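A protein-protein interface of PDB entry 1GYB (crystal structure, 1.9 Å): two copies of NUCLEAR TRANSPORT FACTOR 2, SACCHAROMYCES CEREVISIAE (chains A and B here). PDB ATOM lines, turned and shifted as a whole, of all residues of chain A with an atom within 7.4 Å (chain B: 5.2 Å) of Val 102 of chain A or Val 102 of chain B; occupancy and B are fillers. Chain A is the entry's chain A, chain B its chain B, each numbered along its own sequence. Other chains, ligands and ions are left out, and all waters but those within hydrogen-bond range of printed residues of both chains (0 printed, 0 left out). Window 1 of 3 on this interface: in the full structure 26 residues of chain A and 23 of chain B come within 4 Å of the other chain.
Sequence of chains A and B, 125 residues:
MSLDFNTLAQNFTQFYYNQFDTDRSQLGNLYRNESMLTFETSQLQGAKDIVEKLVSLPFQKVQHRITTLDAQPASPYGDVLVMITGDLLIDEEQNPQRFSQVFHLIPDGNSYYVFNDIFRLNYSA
Among the printed residues, merely in contact across the chains: Gln 72 of chain A with Ile 118 of chain B (3.7 Å), Leu 81 of chain A with Leu 81 of chain B (3.4 Å), Leu 81 of chain A with Val 102 of chain B (3.8 Å), Leu 81 of chain A with Asn 116 of chain B (3.6 Å), Met 83 of chain A with Ser 100 of chain B (3.8 Å), Met 83 of chain A with Val 102 of chain B (3.5 Å), Met 83 of chain A with Ile 118 of chain B (3.6 Å), Ser 100 of chain A with Met 83 of chain B (3.4 Å), Gln 101 of chain A with Met 83 of chain B (3.9 Å), Val 102 of chain A with Val 102 of chain B (3.9 Å), Asn 116 of chain A with Leu 81 of chain B (3.6 Å), Ile 118 of chain A with Met 83 of chain B (3.8 Å) and Arg 120 of chain A with Met 83 of chain B (3.9 Å).
Leu 81 of chain A touches Asn 116 of chain B, and with the chains exchanged Asn 116 of chain A touches Leu 81 of chain B.
Met 83 of chain A touches Val 102 of chain B, but with the chains exchanged Val 102 of chain A does not touch Met 83 of chain B (4.01 Å).
Met 83 of chain A touches Ile 118 of chain B, and with the chains exchanged Ile 118 of chain A touches Met 83 of chain B.
Val 102 of chain A touches its own counterpart, Val 102 of chain B.
12 positions are printed for both chains.
Of the printed residues of chain B, Ser 100 of chain A touches Met 83 (3.4 Å).
Printed residues of chain B within 4 Å of Gln 101 of chain A: Met 83.
Printed residues of chain B within 4 Å of Val 102 of chain A: Val 102.
Of the printed residues of chain A, Leu 81 of chain B touches Leu 81 (3.4 Å) and Asn 116 (3.6 Å).
Of the printed residues of chain A, Asn 116 of chain B touches Gln 72 and Leu 81.
The nearest printed residue of chain B that does not touch Asn 116 of chain A is His 104 of chain B (7.2 Å).
NE2 of Gln 72 of chain A sits at hydrogen-bond distance from O of Asp 117 of chain B (3.2 Å).
The side-chain amide oxygen of Asn 116 of chain B sits close to the side-chain amide oxygen of Gln 72 of chain A (3.0 Å).
Hydrophobic or aromatic side chains of chain B that line the printed part of chain A: Leu 81, Met 83, Val 102 and Ile 118.
Along chain B the printed residues that touch a printed residue of chain A span positions 81 to 118.
Printed residues of chain A that touch a printed residue of chain B: Gln 72, Leu 81, Met 83, Ser 100, Gln 101, Val 102, Asn 116, Ile 118 and Arg 120.
Among the printed residues, no Asp or Glu carboxylate lies within 4 Å of a Lys or Arg side-chain nitrogen of the other chain.
The side-chain amide oxygen of Gln 101 of chain A lies close to the side-chain carboxylate of Asp 117 of chain A, 2.8 Å away.
The side-chain hydroxyl (OH) of Tyr 17 of chain A sits at hydrogen-bond distance from the side-chain amide nitrogen (NE2) of Gln 101 of chain A, 2.6 Å away.
The backbone carbonyl oxygen (O) of Arg 120 of chain A is in hydrogen-bond range of the backbone NH (N) of Ser 100 of chain A, at 2.9 Å.
N of Val 102 of chain B sits at hydrogen-bond distance from O of Ile 118 of chain B.
The backbone NH of His 104 of chain A lies within hydrogen-bond range of the backbone carbonyl oxygen of Asn 116 of chain A (3.0 Å).
OE1 of Gln 101 of chain B sits close to OD1 of Asp 117 of chain B.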
ATOM      1  N   TYR A  17     -17.681 -27.671 -30.762  1.00  0.00           N
ATOM      2  CA  TYR A  17     -18.251 -27.569 -29.428  1.00  0.00           C
ATOM      3  C   TYR A  17     -19.709 -28.001 -29.398  1.00  0.00           C
ATOM      4  O   TYR A  17     -20.179 -28.529 -28.394  1.00  0.00           O
ATOM      5  CB  TYR A  17     -18.086 -26.147 -28.879  1.00  0.00           C
ATOM      6  CG  TYR A  17     -16.639 -25.793 -28.589  1.00  0.00           C
ATOM      7  CD1 TYR A  17     -15.800 -26.698 -27.935  1.00  0.00           C
ATOM      8  CD2 TYR A  17     -16.108 -24.559 -28.967  1.00  0.00           C
ATOM      9  CE1 TYR A  17     -14.465 -26.384 -27.666  1.00  0.00           C
ATOM     10  CE2 TYR A  17     -14.778 -24.235 -28.702  1.00  0.00           C
ATOM     11  CZ  TYR A  17     -13.964 -25.150 -28.052  1.00  0.00           C
ATOM     12  OH  TYR A  17     -12.647 -24.829 -27.795  1.00  0.00           O
ATOM     13  N   MET A  36      -3.078 -35.408 -32.071  1.00  0.00           N
ATOM     14  CA  MET A  36      -2.631 -35.413 -30.685  1.00  0.00           C
ATOM     15  C   MET A  36      -3.505 -34.529 -29.811  1.00  0.00           C
ATOM     16  O   MET A  36      -3.837 -33.402 -30.182  1.00  0.00           O
ATOM     17  CB  MET A  36      -1.191 -34.907 -30.599  1.00  0.00           C
ATOM     18  CG  MET A  36      -0.178 -35.741 -31.367  1.00  0.00           C
ATOM     19  SD  MET A  36       1.368 -34.838 -31.584  1.00  0.00           S
ATOM     20  CE  MET A  36       1.015 -33.913 -33.083  1.00  0.00           C
ATOM     21  N   GLN A  72      -5.257 -17.581 -37.019  1.00  0.00           N
ATOM     22  CA  GLN A  72      -4.232 -17.091 -37.933  1.00  0.00           C
ATOM     23  C   GLN A  72      -3.826 -18.243 -38.827  1.00  0.00           C
ATOM     24  O   GLN A  72      -3.948 -19.404 -38.443  1.00  0.00           O
ATOM     25  CB  GLN A  72      -2.966 -16.649 -37.194  1.00  0.00           C
ATOM     26  CG  GLN A  72      -3.127 -15.645 -36.071  1.00  0.00           C
ATOM     27  CD  GLN A  72      -1.776 -15.263 -35.477  1.00  0.00           C
ATOM     28  OE1 GLN A  72      -0.870 -16.092 -35.394  1.00  0.00           O
ATOM     29  NE2 GLN A  72      -1.638 -14.010 -35.058  1.00  0.00           N
ATOM     30  N   VAL A  80      -4.693 -23.887 -40.300  1.00  0.00           N
ATOM     31  CA  VAL A  80      -5.082 -22.793 -39.423  1.00  0.00           C
ATOM     32  C   VAL A  80      -4.871 -23.055 -37.946  1.00  0.00           C
ATOM     33  O   VAL A  80      -5.059 -24.171 -37.467  1.00  0.00           O
ATOM     34  CB  VAL A  80      -6.574 -22.455 -39.629  1.00  0.00           C
ATOM     35  CG1 VAL A  80      -6.963 -21.246 -38.785  1.00  0.00           C
ATOM     36  CG2 VAL A  80      -6.842 -22.180 -41.111  1.00  0.00           C
ATOM     37  N   LEU A  81      -4.494 -22.001 -37.233  1.00  0.00           N
ATOM     38  CA  LEU A  81      -4.283 -22.071 -35.796  1.00  0.00           C
ATOM     39  C   LEU A  81      -5.441 -21.305 -35.171  1.00  0.00           C
ATOM     40  O   LEU A  81      -5.742 -20.182 -35.582  1.00  0.00           O
ATOM     41  CB  LEU A  81      -2.957 -21.406 -35.424  1.00  0.00           C
ATOM     42  CG  LEU A  81      -2.434 -21.596 -34.000  1.00  0.00           C
ATOM     43  CD1 LEU A  81      -2.346 -23.084 -33.671  1.00  0.00           C
ATOM     44  CD2 LEU A  81      -1.059 -20.940 -33.891  1.00  0.00           C
ATOM     45  N   VAL A  82      -6.099 -21.920 -34.195  1.00  0.00           N
ATOM     46  CA  VAL A  82      -7.231 -21.287 -33.524  1.00  0.00           C
ATOM     47  C   VAL A  82      -7.074 -21.362 -32.007  1.00  0.00           C
ATOM     48  O   VAL A  82      -6.860 -22.446 -31.460  1.00  0.00           O
ATOM     49  CB  VAL A  82      -8.564 -21.991 -33.873  1.00  0.00           C
ATOM     50  CG1 VAL A  82      -9.736 -21.211 -33.265  1.00  0.00           C
ATOM     51  CG2 VAL A  82      -8.718 -22.124 -35.382  1.00  0.00           C
ATOM     52  N   MET A  83      -7.180 -20.218 -31.331  1.00  0.00           N
ATOM     53  CA  MET A  83      -7.096 -20.194 -29.876  1.00  0.00           C
ATOM     54  C   MET A  83      -8.450 -19.787 -29.320  1.00  0.00           C
ATOM     55  O   MET A  83      -9.064 -18.830 -29.794  1.00  0.00           O
ATOM     56  CB  MET A  83      -6.025 -19.216 -29.382  1.00  0.00           C
ATOM     57  CG  MET A  83      -5.903 -19.218 -27.855  1.00  0.00           C
ATOM     58  SD  MET A  83      -4.580 -18.161 -27.206  1.00  0.00           S
ATOM     59  CE  MET A  83      -5.480 -16.589 -26.938  1.00  0.00           C
ATOM     60  N   ILE A  84      -8.913 -20.520 -28.316  1.00  0.00           N
ATOM     61  CA  ILE A  84     -10.205 -20.243 -27.701  1.00  0.00           C
ATOM     62  C   ILE A  84     -10.090 -20.118 -26.183  1.00  0.00           C
ATOM     63  O   ILE A  84      -9.332 -20.850 -25.552  1.00  0.00           O
ATOM     64  CB  ILE A  84     -11.214 -21.395 -27.970  1.00  0.00           C
ATOM     65  CG1 ILE A  84     -11.330 -21.665 -29.466  1.00  0.00           C
ATOM     66  CG2 ILE A  84     -12.574 -21.066 -27.375  1.00  0.00           C
ATOM     67  CD1 ILE A  84     -10.374 -22.748 -29.955  1.00  0.00           C
ATOM     68  N   PHE A  99     -11.636 -22.133 -19.331  1.00  0.00           N
ATOM     69  CA  PHE A  99     -10.838 -23.045 -20.138  1.00  0.00           C
ATOM     70  C   PHE A  99     -10.144 -22.291 -21.276  1.00  0.00           C
ATOM     71  O   PHE A  99     -10.565 -21.204 -21.670  1.00  0.00           O
ATOM     72  CB  PHE A  99     -11.722 -24.163 -20.704  1.00  0.00           C
ATOM     73  CG  PHE A  99     -12.502 -23.769 -21.928  1.00  0.00           C
ATOM     74  CD1 PHE A  99     -11.924 -23.858 -23.192  1.00  0.00           C
ATOM     75  CD2 PHE A  99     -13.807 -23.300 -21.816  1.00  0.00           C
ATOM     76  CE1 PHE A  99     -12.640 -23.483 -24.339  1.00  0.00           C
ATOM     77  CE2 PHE A  99     -14.532 -22.922 -22.953  1.00  0.00           C
ATOM     78  CZ  PHE A  99     -13.944 -23.016 -24.215  1.00  0.00           C
ATOM     79  N   SER A 100      -9.053 -22.861 -21.772  1.00  0.00           N
ATOM     80  CA  SER A 100      -8.325 -22.285 -22.891  1.00  0.00           C
ATOM     81  C   SER A 100      -8.037 -23.476 -23.804  1.00  0.00           C
ATOM     82  O   SER A 100      -7.781 -24.584 -23.327  1.00  0.00           O
ATOM     83  CB  SER A 100      -7.027 -21.620 -22.415  1.00  0.00           C
ATOM     84  OG  SER A 100      -6.228 -22.538 -21.694  1.00  0.00           O
ATOM     85  N   GLN A 101      -8.116 -23.269 -25.113  1.00  0.00           N
ATOM     86  CA  GLN A 101      -7.880 -24.372 -26.042  1.00  0.00           C
ATOM     87  C   GLN A 101      -7.286 -23.868 -27.338  1.00  0.00           C
ATOM     88  O   GLN A 101      -7.595 -22.763 -27.780  1.00  0.00           O
ATOM     89  CB  GLN A 101      -9.201 -25.109 -26.338  1.00  0.00           C
ATOM     90  CG  GLN A 101      -9.038 -26.402 -27.153  1.00  0.00           C
ATOM     91  CD  GLN A 101     -10.202 -27.381 -26.985  1.00  0.00           C
ATOM     92  OE1 GLN A 101     -10.026 -28.595 -27.101  1.00  0.00           O
ATOM     93  NE2 GLN A 101     -11.387 -26.855 -26.724  1.00  0.00           N
ATOM     94  N   VAL A 102      -6.405 -24.667 -27.929  1.00  0.00           N
ATOM     95  CA  VAL A 102      -5.822 -24.309 -29.204  1.00  0.00           C
ATOM     96  C   VAL A 102      -5.962 -25.504 -30.137  1.00  0.00           C
ATOM     97  O   VAL A 102      -5.756 -26.649 -29.738  1.00  0.00           O
ATOM     98  CB  VAL A 102      -4.323 -23.878 -29.082  1.00  0.00           C
ATOM     99  CG1 VAL A 102      -3.486 -24.972 -28.443  1.00  0.00           C
ATOM    100  CG2 VAL A 102      -3.777 -23.551 -30.463  1.00  0.00           C
ATOM    101  N   PHE A 103      -6.363 -25.228 -31.372  1.00  0.00           N
ATOM    102  CA  PHE A 103      -6.509 -26.263 -32.387  1.00  0.00           C
ATOM    103  C   PHE A 103      -5.617 -25.902 -33.565  1.00  0.00           C
ATOM    104  O   PHE A 103      -5.497 -24.730 -33.912  1.00  0.00           O
ATOM    105  CB  PHE A 103      -7.942 -26.319 -32.940  1.00  0.00           C
ATOM    106  CG  PHE A 103      -8.976 -26.782 -31.956  1.00  0.00           C
ATOM    107  CD1 PHE A 103      -9.965 -25.911 -31.513  1.00  0.00           C
ATOM    108  CD2 PHE A 103      -8.996 -28.097 -31.519  1.00  0.00           C
ATOM    109  CE1 PHE A 103     -10.970 -26.343 -30.651  1.00  0.00           C
ATOM    110  CE2 PHE A 103      -9.994 -28.542 -30.658  1.00  0.00           C
ATOM    111  CZ  PHE A 103     -10.987 -27.659 -30.224  1.00  0.00           C
ATOM    112  N   HIS A 104      -4.990 -26.907 -34.168  1.00  0.00           N
ATOM    113  CA  HIS A 104      -4.194 -26.695 -35.373  1.00  0.00           C
ATOM    114  C   HIS A 104      -5.031 -27.502 -36.366  1.00  0.00           C
ATOM    115  O   HIS A 104      -5.107 -28.735 -36.281  1.00  0.00           O
ATOM    116  CB  HIS A 104      -2.783 -27.274 -35.216  1.00  0.00           C
ATOM    117  CG  HIS A 104      -1.924 -27.143 -36.442  1.00  0.00           C
ATOM    118  ND1 HIS A 104      -2.206 -26.271 -37.465  1.00  0.00           N
ATOM    119  CD2 HIS A 104      -0.772 -27.773 -36.783  1.00  0.00           C
ATOM    120  CE1 HIS A 104      -1.262 -26.365 -38.394  1.00  0.00           C
ATOM    121  NE2 HIS A 104      -0.386 -27.267 -38.001  1.00  0.00           N
ATOM    122  N   LEU A 105      -5.702 -26.786 -37.264  1.00  0.00           N
ATOM    123  CA  LEU A 105      -6.590 -27.397 -38.252  1.00  0.00           C
ATOM    124  C   LEU A 105      -5.905 -27.611 -39.591  1.00  0.00           C
ATOM    125  O   LEU A 105      -5.267 -26.702 -40.121  1.00  0.00           O
ATOM    126  CB  LEU A 105      -7.826 -26.513 -38.444  1.00  0.00           C
ATOM    127  CG  LEU A 105      -8.612 -26.176 -37.175  1.00  0.00           C
ATOM    128  CD1 LEU A 105      -9.847 -25.357 -37.542  1.00  0.00           C
ATOM    129  CD2 LEU A 105      -9.008 -27.463 -36.455  1.00  0.00           C
ATOM    130  N   VAL A 114      -8.523 -32.051 -36.953  1.00  0.00           N
ATOM    131  CA  VAL A 114      -7.651 -31.546 -35.904  1.00  0.00           C
ATOM    132  C   VAL A 114      -6.356 -32.333 -35.792  1.00  0.00           C
ATOM    133  O   VAL A 114      -6.366 -33.536 -35.530  1.00  0.00           O
ATOM    134  CB  VAL A 114      -8.373 -31.584 -34.548  1.00  0.00           C
ATOM    135  CG1 VAL A 114      -7.462 -31.068 -33.448  1.00  0.00           C
ATOM    136  CG2 VAL A 114      -9.654 -30.764 -34.621  1.00  0.00           C
ATOM    137  N   ASN A 116      -3.587 -30.823 -33.954  1.00  0.00           N
ATOM    138  CA  ASN A 116      -3.185 -30.492 -32.581  1.00  0.00           C
ATOM    139  C   ASN A 116      -4.393 -30.020 -31.795  1.00  0.00           C
ATOM    140  O   ASN A 116      -5.163 -29.185 -32.266  1.00  0.00           O
ATOM    141  CB  ASN A 116      -2.163 -29.345 -32.524  1.00  0.00           C
ATOM    142  CG  ASN A 116      -0.843 -29.679 -33.176  1.00  0.00           C
ATOM    143  OD1 ASN A 116      -0.109 -30.565 -32.724  1.00  0.00           O
ATOM    144  ND2 ASN A 116      -0.516 -28.954 -34.235  1.00  0.00           N
ATOM    145  N   ASP A 117      -4.539 -30.544 -30.586  1.00  0.00           N
ATOM    146  CA  ASP A 117      -5.624 -30.156 -29.701  1.00  0.00           C
ATOM    147  C   ASP A 117      -5.002 -30.039 -28.310  1.00  0.00           C
ATOM    148  O   ASP A 117      -4.595 -31.045 -27.730  1.00  0.00           O
ATOM    149  CB  ASP A 117      -6.713 -31.232 -29.685  1.00  0.00           C
ATOM    150  CG  ASP A 117      -7.907 -30.844 -28.832  1.00  0.00           C
ATOM    151  OD1 ASP A 117      -7.771 -29.936 -27.978  1.00  0.00           O
ATOM    152  OD2 ASP A 117      -8.984 -31.456 -29.007  1.00  0.00           O
ATOM    153  N   ILE A 118      -4.897 -28.819 -27.789  1.00  0.00           N
ATOM    154  CA  ILE A 118      -4.337 -28.613 -26.450  1.00  0.00           C
ATOM    155  C   ILE A 118      -5.434 -27.951 -25.620  1.00  0.00           C
ATOM    156  O   ILE A 118      -5.934 -26.890 -25.981  1.00  0.00           O
ATOM    157  CB  ILE A 118      -3.067 -27.716 -26.484  1.00  0.00           C
ATOM    158  CG1 ILE A 118      -2.005 -28.351 -27.401  1.00  0.00           C
ATOM    159  CG2 ILE A 118      -2.493 -27.575 -25.063  1.00  0.00           C
ATOM    160  CD1 ILE A 118      -0.708 -27.542 -27.547  1.00  0.00           C
ATOM    161  N   PHE A 119      -5.810 -28.594 -24.518  1.00  0.00           N
ATOM    162  CA  PHE A 119      -6.885 -28.105 -23.656  1.00  0.00           C
ATOM    163  C   PHE A 119      -6.481 -27.990 -22.187  1.00  0.00           C
ATOM    164  O   PHE A 119      -5.832 -28.881 -21.632  1.00  0.00           O
ATOM    165  CB  PHE A 119      -8.087 -29.046 -23.778  1.00  0.00           C
ATOM    166  CG  PHE A 119      -9.217 -28.724 -22.836  1.00  0.00           C
ATOM    167  CD1 PHE A 119     -10.166 -27.757 -23.162  1.00  0.00           C
ATOM    168  CD2 PHE A 119      -9.329 -29.389 -21.621  1.00  0.00           C
ATOM    169  CE1 PHE A 119     -11.209 -27.460 -22.293  1.00  0.00           C
ATOM    170  CE2 PHE A 119     -10.375 -29.097 -20.736  1.00  0.00           C
ATOM    171  CZ  PHE A 119     -11.313 -28.132 -21.074  1.00  0.00           C
ATOM    172  N   ARG A 120      -6.901 -26.901 -21.557  1.00  0.00           N
ATOM    173  CA  ARG A 120      -6.590 -26.656 -20.155  1.00  0.00           C
ATOM    174  C   ARG A 120      -7.684 -25.885 -19.431  1.00  0.00           C
ATOM    175  O   ARG A 120      -8.309 -24.984 -20.002  1.00  0.00           O
ATOM    176  CB  ARG A 120      -5.297 -25.840 -20.038  1.00  0.00           C
ATOM    177  CG  ARG A 120      -4.028 -26.646 -20.039  1.00  0.00           C
ATOM    178  CD  ARG A 120      -3.754 -27.195 -18.654  1.00  0.00           C
ATOM    179  NE  ARG A 120      -2.553 -28.014 -18.627  1.00  0.00           N
ATOM    180  CZ  ARG A 120      -2.084 -28.605 -17.536  1.00  0.00           C
ATOM    181  NH1 ARG A 120      -2.721 -28.461 -16.382  1.00  0.00           N
ATOM    182  NH2 ARG A 120      -0.980 -29.341 -17.601  1.00  0.00           N
ATOM    183  N   LEU B  81       4.119 -26.184 -31.209  1.00  0.00           N
ATOM    184  CA  LEU B  81       2.956 -25.391 -30.823  1.00  0.00           C
ATOM    185  C   LEU B  81       2.930 -25.410 -29.296  1.00  0.00           C
ATOM    186  O   LEU B  81       3.033 -26.472 -28.684  1.00  0.00           O
ATOM    187  CB  LEU B  81       1.669 -26.020 -31.362  1.00  0.00           C
ATOM    188  CG  LEU B  81       0.364 -25.262 -31.105  1.00  0.00           C
ATOM    189  CD1 LEU B  81       0.376 -23.968 -31.889  1.00  0.00           C
ATOM    190  CD2 LEU B  81      -0.830 -26.130 -31.517  1.00  0.00           C
ATOM    191  N   VAL B  82       2.807 -24.240 -28.683  1.00  0.00           N
ATOM    192  CA  VAL B  82       2.776 -24.166 -27.232  1.00  0.00           C
ATOM    193  C   VAL B  82       1.666 -23.230 -26.782  1.00  0.00           C
ATOM    194  O   VAL B  82       1.452 -22.174 -27.385  1.00  0.00           O
ATOM    195  CB  VAL B  82       4.135 -23.656 -26.682  1.00  0.00           C
ATOM    196  CG1 VAL B  82       4.511 -22.353 -27.365  1.00  0.00           C
ATOM    197  CG2 VAL B  82       4.061 -23.464 -25.166  1.00  0.00           C
ATOM    198  N   MET B  83       0.928 -23.637 -25.751  1.00  0.00           N
ATOM    199  CA  MET B  83      -0.126 -22.791 -25.210  1.00  0.00           C
ATOM    200  C   MET B  83       0.262 -22.478 -23.773  1.00  0.00           C
ATOM    201  O   MET B  83       0.621 -23.369 -23.007  1.00  0.00           O
ATOM    202  CB  MET B  83      -1.484 -23.487 -25.243  1.00  0.00           C
ATOM    203  CG  MET B  83      -2.572 -22.624 -24.618  1.00  0.00           C
ATOM    204  SD  MET B  83      -4.238 -23.264 -24.858  1.00  0.00           S
ATOM    205  CE  MET B  83      -4.272 -24.492 -23.601  1.00  0.00           C
ATOM    206  N   ILE B  84       0.178 -21.206 -23.415  1.00  0.00           N
ATOM    207  CA  ILE B  84       0.568 -20.755 -22.091  1.00  0.00           C
ATOM    208  C   ILE B  84      -0.497 -19.918 -21.404  1.00  0.00           C
ATOM    209  O   ILE B  84      -1.173 -19.118 -22.044  1.00  0.00           O
ATOM    210  CB  ILE B  84       1.831 -19.880 -22.196  1.00  0.00           C
ATOM    211  CG1 ILE B  84       3.021 -20.740 -22.606  1.00  0.00           C
ATOM    212  CG2 ILE B  84       2.086 -19.140 -20.888  1.00  0.00           C
ATOM    213  CD1 ILE B  84       4.279 -19.954 -22.792  1.00  0.00           C
ATOM    214  N   SER B 100      -3.557 -15.601 -21.667  1.00  0.00           N
ATOM    215  CA  SER B 100      -3.399 -16.892 -22.331  1.00  0.00           C
ATOM    216  C   SER B 100      -2.666 -16.559 -23.625  1.00  0.00           C
ATOM    217  O   SER B 100      -2.970 -15.557 -24.274  1.00  0.00           O
ATOM    218  CB  SER B 100      -4.754 -17.547 -22.634  1.00  0.00           C
ATOM    219  OG  SER B 100      -5.340 -18.071 -21.455  1.00  0.00           O
ATOM    220  N   GLN B 101      -1.698 -17.386 -24.000  1.00  0.00           N
ATOM    221  CA  GLN B 101      -0.928 -17.122 -25.204  1.00  0.00           C
ATOM    222  C   GLN B 101      -0.568 -18.396 -25.956  1.00  0.00           C
ATOM    223  O   GLN B 101      -0.360 -19.442 -25.349  1.00  0.00           O
ATOM    224  CB  GLN B 101       0.355 -16.355 -24.828  1.00  0.00           C
ATOM    225  CG  GLN B 101       1.235 -15.950 -26.001  1.00  0.00           C
ATOM    226  CD  GLN B 101       2.114 -14.747 -25.680  1.00  0.00           C
ATOM    227  OE1 GLN B 101       2.295 -13.862 -26.513  1.00  0.00           O
ATOM    228  NE2 GLN B 101       2.659 -14.712 -24.472  1.00  0.00           N
ATOM    229  N   VAL B 102      -0.524 -18.307 -27.281  1.00  0.00           N
ATOM    230  CA  VAL B 102      -0.138 -19.453 -28.101  1.00  0.00           C
ATOM    231  C   VAL B 102       0.983 -19.011 -29.037  1.00  0.00           C
ATOM    232  O   VAL B 102       0.925 -17.924 -29.606  1.00  0.00           O
ATOM    233  CB  VAL B 102      -1.326 -19.986 -28.956  1.00  0.00           C
ATOM    234  CG1 VAL B 102      -0.812 -20.922 -30.049  1.00  0.00           C
ATOM    235  CG2 VAL B 102      -2.320 -20.721 -28.064  1.00  0.00           C
ATOM    236  N   PHE B 103       2.018 -19.837 -29.166  1.00  0.00           N
ATOM    237  CA  PHE B 103       3.119 -19.542 -30.073  1.00  0.00           C
ATOM    238  C   PHE B 103       3.269 -20.726 -31.014  1.00  0.00           C
ATOM    239  O   PHE B 103       3.107 -21.869 -30.595  1.00  0.00           O
ATOM    240  CB  PHE B 103       4.476 -19.438 -29.362  1.00  0.00           C
ATOM    241  CG  PHE B 103       4.637 -18.238 -28.483  1.00  0.00           C
ATOM    242  CD1 PHE B 103       4.783 -18.397 -27.111  1.00  0.00           C
ATOM    243  CD2 PHE B 103       4.714 -16.958 -29.025  1.00  0.00           C
ATOM    244  CE1 PHE B 103       5.011 -17.301 -26.288  1.00  0.00           C
ATOM    245  CE2 PHE B 103       4.942 -15.852 -28.206  1.00  0.00           C
ATOM    246  CZ  PHE B 103       5.092 -16.032 -26.838  1.00  0.00           C
ATOM    247  N   HIS B 104       3.579 -20.446 -32.275  1.00  0.00           N
ATOM    248  CA  HIS B 104       3.881 -21.500 -33.243  1.00  0.00           C
ATOM    249  C   HIS B 104       5.363 -21.191 -33.472  1.00  0.00           C
ATOM    250  O   HIS B 104       5.704 -20.145 -34.033  1.00  0.00           O
ATOM    251  CB  HIS B 104       3.100 -21.329 -34.547  1.00  0.00           C
ATOM    252  CG  HIS B 104       3.418 -22.369 -35.579  1.00  0.00           C
ATOM    253  ND1 HIS B 104       2.931 -22.315 -36.869  1.00  0.00           N
ATOM    254  CD2 HIS B 104       4.178 -23.488 -35.513  1.00  0.00           C
ATOM    255  CE1 HIS B 104       3.379 -23.355 -37.550  1.00  0.00           C
ATOM    256  NE2 HIS B 104       4.138 -24.083 -36.751  1.00  0.00           N
ATOM    257  N   ASN B 116       3.645 -17.643 -35.349  1.00  0.00           N
ATOM    258  CA  ASN B 116       2.301 -17.298 -34.887  1.00  0.00           C
ATOM    259  C   ASN B 116       2.366 -16.919 -33.412  1.00  0.00           C
ATOM    260  O   ASN B 116       2.973 -17.620 -32.600  1.00  0.00           O
ATOM    261  CB  ASN B 116       1.333 -18.479 -35.029  1.00  0.00           C
ATOM    262  CG  ASN B 116       1.072 -18.851 -36.467  1.00  0.00           C
ATOM    263  OD1 ASN B 116       0.370 -18.140 -37.193  1.00  0.00           O
ATOM    264  ND2 ASN B 116       1.639 -19.970 -36.891  1.00  0.00           N
ATOM    265  N   ASP B 117       1.728 -15.806 -33.075  1.00  0.00           N
ATOM    266  CA  ASP B 117       1.680 -15.316 -31.705  1.00  0.00           C
ATOM    267  C   ASP B 117       0.250 -14.819 -31.507  1.00  0.00           C
ATOM    268  O   ASP B 117      -0.176 -13.880 -32.179  1.00  0.00           O
ATOM    269  CB  ASP B 117       2.668 -14.152 -31.520  1.00  0.00           C
ATOM    270  CG  ASP B 117       2.743 -13.665 -30.072  1.00  0.00           C
ATOM    271  OD1 ASP B 117       1.780 -13.899 -29.307  1.00  0.00           O
ATOM    272  OD2 ASP B 117       3.759 -13.031 -29.697  1.00  0.00           O
ATOM    273  N   ILE B 118      -0.494 -15.471 -30.615  1.00  0.00           N
ATOM    274  CA  ILE B 118      -1.874 -15.080 -30.321  1.00  0.00           C
ATOM    275  C   ILE B 118      -1.939 -14.772 -28.834  1.00  0.00           C
ATOM    276  O   ILE B 118      -1.614 -15.620 -28.007  1.00  0.00           O
ATOM    277  CB  ILE B 118      -2.878 -16.211 -30.643  1.00  0.00           C
ATOM    278  CG1 ILE B 118      -2.863 -16.510 -32.148  1.00  0.00           C
ATOM    279  CG2 ILE B 118      -4.294 -15.786 -30.215  1.00  0.00           C
ATOM    280  CD1 ILE B 118      -3.843 -17.592 -32.558  1.00  0.00           C
